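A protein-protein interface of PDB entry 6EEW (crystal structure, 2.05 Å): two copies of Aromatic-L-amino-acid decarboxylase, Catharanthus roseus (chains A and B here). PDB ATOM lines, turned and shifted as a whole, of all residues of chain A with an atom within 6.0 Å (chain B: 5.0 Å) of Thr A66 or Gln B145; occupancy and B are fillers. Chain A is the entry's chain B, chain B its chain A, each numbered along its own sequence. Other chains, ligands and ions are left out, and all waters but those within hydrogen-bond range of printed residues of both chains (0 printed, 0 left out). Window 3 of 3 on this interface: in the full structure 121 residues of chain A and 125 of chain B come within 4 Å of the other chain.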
ATOM      1  N   PRO A  64     -11.188   7.232  14.212  1.00  0.00           N
ATOM      2  CA  PRO A  64     -11.552   8.431  13.442  1.00  0.00           C
ATOM      3  C   PRO A  64     -12.458   8.095  12.262  1.00  0.00           C
ATOM      4  O   PRO A  64     -12.471   6.973  11.744  1.00  0.00           O
ATOM      5  CB  PRO A  64     -10.195   8.982  12.982  1.00  0.00           C
ATOM      6  CG  PRO A  64      -9.226   8.488  14.045  1.00  0.00           C
ATOM      7  CD  PRO A  64      -9.729   7.110  14.406  1.00  0.00           C
ATOM      8  N   GLU A  65     -13.244   9.091  11.854  1.00  0.00           N
ATOM      9  CA  GLU A  65     -14.196   8.909  10.768  1.00  0.00           C
ATOM     10  C   GLU A  65     -13.547   8.874   9.390  1.00  0.00           C
ATOM     11  O   GLU A  65     -14.199   8.440   8.427  1.00  0.00           O
ATOM     12  CB  GLU A  65     -15.256  10.006  10.828  1.00  0.00           C
ATOM     13  CG  GLU A  65     -16.213   9.846  12.005  1.00  0.00           C
ATOM     14  CD  GLU A  65     -17.199  10.992  12.130  1.00  0.00           C
ATOM     15  OE1 GLU A  65     -17.156  11.916  11.284  1.00  0.00           O
ATOM     16  OE2 GLU A  65     -18.013  10.972  13.083  1.00  0.00           O
ATOM     17  N   THR A  66     -12.301   9.314   9.243  1.00  0.00           N
ATOM     18  CA  THR A  66     -11.673   9.211   7.935  1.00  0.00           C
ATOM     19  C   THR A  66     -10.277   8.643   8.093  1.00  0.00           C
ATOM     20  O   THR A  66      -9.644   8.786   9.139  1.00  0.00           O
ATOM     21  CB  THR A  66     -11.611  10.560   7.181  1.00  0.00           C
ATOM     22  OG1 THR A  66     -10.593  11.400   7.728  1.00  0.00           O
ATOM     23  CG2 THR A  66     -12.943  11.265   7.268  1.00  0.00           C
ATOM     24  N   ALA A  67      -9.791   8.039   7.010  1.00  0.00           N
ATOM     25  CA  ALA A  67      -8.453   7.474   7.011  1.00  0.00           C
ATOM     26  C   ALA A  67      -7.402   8.576   7.095  1.00  0.00           C
ATOM     27  O   ALA A  67      -7.619   9.705   6.634  1.00  0.00           O
ATOM     28  CB  ALA A  67      -8.220   6.631   5.757  1.00  0.00           C
ATOM     29  N   PRO A  68      -6.250   8.277   7.675  1.00  0.00           N
ATOM     30  CA  PRO A  68      -5.236   9.318   7.853  1.00  0.00           C
ATOM     31  C   PRO A  68      -4.516   9.640   6.554  1.00  0.00           C
ATOM     32  O   PRO A  68      -4.144   8.751   5.783  1.00  0.00           O
ATOM     33  CB  PRO A  68      -4.281   8.707   8.885  1.00  0.00           C
ATOM     34  CG  PRO A  68      -4.426   7.241   8.714  1.00  0.00           C
ATOM     35  CD  PRO A  68      -5.884   7.014   8.341  1.00  0.00           C
ATOM     36  N   TYR A  69      -4.327  10.944   6.320  1.00  0.00           N
ATOM     37  CA  TYR A  69      -3.496  11.377   5.207  1.00  0.00           C
ATOM     38  C   TYR A  69      -2.078  10.865   5.367  1.00  0.00           C
ATOM     39  O   TYR A  69      -1.478  10.364   4.405  1.00  0.00           O
ATOM     40  CB  TYR A  69      -3.522  12.907   5.096  1.00  0.00           C
ATOM     41  CG  TYR A  69      -4.791  13.373   4.437  1.00  0.00           C
ATOM     42  CD1 TYR A  69      -4.995  13.155   3.084  1.00  0.00           C
ATOM     43  CD2 TYR A  69      -5.802  13.984   5.166  1.00  0.00           C
ATOM     44  CE1 TYR A  69      -6.156  13.545   2.469  1.00  0.00           C
ATOM     45  CE2 TYR A  69      -6.974  14.386   4.551  1.00  0.00           C
ATOM     46  CZ  TYR A  69      -7.142  14.162   3.199  1.00  0.00           C
ATOM     47  OH  TYR A  69      -8.300  14.548   2.562  1.00  0.00           O
ATOM     48  N   ASP B 141     -16.329   2.660   5.005  1.00  0.00           N
ATOM     49  CA  ASP B 141     -16.637   4.084   4.901  1.00  0.00           C
ATOM     50  C   ASP B 141     -15.366   4.925   4.680  1.00  0.00           C
ATOM     51  O   ASP B 141     -15.377   5.895   3.903  1.00  0.00           O
ATOM     52  CB  ASP B 141     -17.390   4.539   6.153  1.00  0.00           C
ATOM     53  CG  ASP B 141     -18.901   4.272   6.074  1.00  0.00           C
ATOM     54  OD1 ASP B 141     -19.359   3.599   5.128  1.00  0.00           O
ATOM     55  OD2 ASP B 141     -19.638   4.741   6.970  1.00  0.00           O
ATOM     56  N   TRP B 142     -14.258   4.563   5.335  1.00  0.00           N
ATOM     57  CA  TRP B 142     -12.969   5.199   5.053  1.00  0.00           C
ATOM     58  C   TRP B 142     -12.647   5.144   3.576  1.00  0.00           C
ATOM     59  O   TRP B 142     -12.362   6.161   2.934  1.00  0.00           O
ATOM     60  CB  TRP B 142     -11.843   4.494   5.805  1.00  0.00           C
ATOM     61  CG  TRP B 142     -11.666   4.922   7.191  1.00  0.00           C
ATOM     62  CD1 TRP B 142     -12.568   5.568   7.963  1.00  0.00           C
ATOM     63  CD2 TRP B 142     -10.509   4.714   7.997  1.00  0.00           C
ATOM     64  NE1 TRP B 142     -12.044   5.789   9.222  1.00  0.00           N
ATOM     65  CE2 TRP B 142     -10.774   5.278   9.262  1.00  0.00           C
ATOM     66  CE3 TRP B 142      -9.265   4.121   7.767  1.00  0.00           C
ATOM     67  CZ2 TRP B 142      -9.843   5.265  10.298  1.00  0.00           C
ATOM     68  CZ3 TRP B 142      -8.333   4.106   8.795  1.00  0.00           C
ATOM     69  CH2 TRP B 142      -8.626   4.680  10.047  1.00  0.00           C
ATOM     70  N   LEU B 143     -12.657   3.932   3.030  1.00  0.00           N
ATOM     71  CA  LEU B 143     -12.276   3.759   1.641  1.00  0.00           C
ATOM     72  C   LEU B 143     -13.240   4.486   0.724  1.00  0.00           C
ATOM     73  O   LEU B 143     -12.821   5.140  -0.237  1.00  0.00           O
ATOM     74  CB  LEU B 143     -12.200   2.278   1.327  1.00  0.00           C
ATOM     75  CG  LEU B 143     -11.097   1.838   0.385  1.00  0.00           C
ATOM     76  CD1 LEU B 143      -9.823   2.527   0.753  1.00  0.00           C
ATOM     77  CD2 LEU B 143     -10.943   0.324   0.543  1.00  0.00           C
ATOM     78  N   ALA B 144     -14.536   4.427   1.037  1.00  0.00           N
ATOM     79  CA  ALA B 144     -15.516   5.134   0.229  1.00  0.00           C
ATOM     80  C   ALA B 144     -15.196   6.622   0.167  1.00  0.00           C
ATOM     81  O   ALA B 144     -15.330   7.249  -0.894  1.00  0.00           O
ATOM     82  CB  ALA B 144     -16.914   4.907   0.800  1.00  0.00           C
ATOM     83  N   GLN B 145     -14.792   7.206   1.302  1.00  0.00           N
ATOM     84  CA  GLN B 145     -14.445   8.624   1.321  1.00  0.00           C
ATOM     85  C   GLN B 145     -13.172   8.904   0.532  1.00  0.00           C
ATOM     86  O   GLN B 145     -13.080   9.922  -0.171  1.00  0.00           O
ATOM     87  CB  GLN B 145     -14.267   9.111   2.755  1.00  0.00           C
ATOM     88  CG  GLN B 145     -15.498   9.031   3.615  1.00  0.00           C
ATOM     89  CD  GLN B 145     -15.167   9.351   5.059  1.00  0.00           C
ATOM     90  OE1 GLN B 145     -14.958  10.508   5.402  1.00  0.00           O
ATOM     91  NE2 GLN B 145     -15.063   8.324   5.897  1.00  0.00           N
ATOM     92  N   ILE B 146     -12.158   8.042   0.655  1.00  0.00           N
ATOM     93  CA  ILE B 146     -10.965   8.258  -0.159  1.00  0.00           C
ATOM     94  C   ILE B 146     -11.354   8.244  -1.629  1.00  0.00           C
ATOM     95  O   ILE B 146     -10.919   9.091  -2.415  1.00  0.00           O
ATOM     96  CB  ILE B 146      -9.882   7.208   0.157  1.00  0.00           C
ATOM     97  CG1 ILE B 146      -9.345   7.382   1.579  1.00  0.00           C
ATOM     98  CG2 ILE B 146      -8.710   7.340  -0.785  1.00  0.00           C
ATOM     99  CD1 ILE B 146      -8.797   6.088   2.152  1.00  0.00           C
ATOM    100  N   LEU B 147     -12.219   7.308  -2.014  1.00  0.00           N
ATOM    101  CA  LEU B 147     -12.701   7.284  -3.386  1.00  0.00           C
ATOM    102  C   LEU B 147     -13.651   8.421  -3.680  1.00  0.00           C
ATOM    103  O   LEU B 147     -14.100   8.536  -4.826  1.00  0.00           O
ATOM    104  CB  LEU B 147     -13.383   5.946  -3.676  1.00  0.00           C
ATOM    105  CG  LEU B 147     -12.471   4.716  -3.561  1.00  0.00           C
ATOM    106  CD1 LEU B 147     -13.275   3.396  -3.580  1.00  0.00           C
ATOM    107  CD2 LEU B 147     -11.389   4.742  -4.635  1.00  0.00           C
ATOM    108  N   LYS B 148     -13.985   9.241  -2.676  1.00  0.00           N
ATOM    109  CA  LYS B 148     -14.914  10.364  -2.842  1.00  0.00           C
ATOM    110  C   LYS B 148     -16.241   9.913  -3.439  1.00  0.00           C
ATOM    111  O   LYS B 148     -16.802  10.560  -4.330  1.00  0.00           O
ATOM    112  CB  LYS B 148     -14.298  11.503  -3.667  1.00  0.00           C
ATOM    113  CG  LYS B 148     -13.112  12.209  -2.990  1.00  0.00           C
ATOM    114  CD  LYS B 148     -12.538  13.291  -3.878  1.00  0.00           C
ATOM    115  CE  LYS B 148     -11.255  13.898  -3.308  1.00  0.00           C
ATOM    116  NZ  LYS B 148     -11.437  14.504  -1.947  1.00  0.00           N
ATOM    117  N   LEU B 149     -16.758   8.803  -2.918  1.00  0.00           N
ATOM    118  CA  LEU B 149     -18.081   8.337  -3.279  1.00  0.00           C
ATOM    119  C   LEU B 149     -19.143   9.121  -2.507  1.00  0.00           C
ATOM    120  O   LEU B 149     -18.898   9.594  -1.392  1.00  0.00           O
ATOM    121  CB  LEU B 149     -18.225   6.851  -2.958  1.00  0.00           C
ATOM    122  CG  LEU B 149     -17.180   5.894  -3.536  1.00  0.00           C
ATOM    123  CD1 LEU B 149     -17.514   4.458  -3.129  1.00  0.00           C
ATOM    124  CD2 LEU B 149     -17.106   6.026  -5.061  1.00  0.00           C
ATOM    125  N   MET B 154     -22.397   4.806   1.833  1.00  0.00           N
ATOM    126  CA  MET B 154     -21.738   4.705   3.126  1.00  0.00           C
ATOM    127  C   MET B 154     -22.711   4.282   4.208  1.00  0.00           C
ATOM    128  O   MET B 154     -23.883   4.677   4.211  1.00  0.00           O
ATOM    129  CB  MET B 154     -21.093   6.041   3.539  1.00  0.00           C
ATOM    130  CG  MET B 154     -20.118   6.554   2.544  1.00  0.00           C
ATOM    131  SD  MET B 154     -19.376   8.118   3.030  1.00  0.00           S
ATOM    132  CE  MET B 154     -18.413   8.426   1.553  1.00  0.00           C
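Among the printed residues, merely in contact across the chains: Glu A65 with Trp B142 (3.3 Å), Thr A66 with Trp B142 (3.5 Å), Thr A66 with Gln B145 (2.8 Å), Ala A67 with Trp B142 (3.4 Å), Ala A67 with Ile B146 (3.7 Å) and Pro A68 with Trp B142 (3.8 Å).
O of Asp B141 lies close to NE2 of Gln B145, at 3.2 Å.
Of the 10 printed residues of chain B, 3 touch a printed residue of chain A. Hydrophobic or aromatic side chains of chain B within 4 Å of the printed part of chain A: Trp B142 and Ile B146. Hydrophobic or aromatic side chains of chain A within 4 Å of the printed part of chain B: Ala A67 and Pro A68. Among the printed residues, 8 pairs touch across the chains. Among the printed residues, no Asp or Glu carboxylate lies within 4 Å of a Lys or Arg side-chain nitrogen of the other chain.
Thr A66 touches two residues of chain B. Printed residues of chain B within 4 Å of Ala A67: Trp B142 (3.4 Å) and Ile B146 (3.7 Å). Printed residues of chain B within 4 Å of Pro A68: Trp B142. Of the printed residues of chain A, Trp B142 touches Pro A64 (2.8 Å), Glu A65 (3.3 Å), Thr A66 (3.5 Å), Ala A67 (3.4 Å) and Pro A68 (3.8 Å). Of chain A, only Glu A65 and Thr A66 come within 4 Å of Gln B145. Of the printed residues of chain A, Ile B146 touches Ala A67. Lys B148 touches none of the printed residues of chain A. The nearest printed residue of chain B that does not touch Ala A67 is Gln B145 (5.4 Å).
No position is printed for both chains. Of the 8 pairs that touch across the chains among the printed residues, none has its exchanged pair printed and touching as well.
The side-chain amide nitrogen of Gln B145 sits at hydrogen-bond distance from the backbone carbonyl oxygen of Glu A65. The indole nitrogen of Trp B142 is in hydrogen-bond range of the backbone carbonyl oxygen of Pro A64 (2.8 Å).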
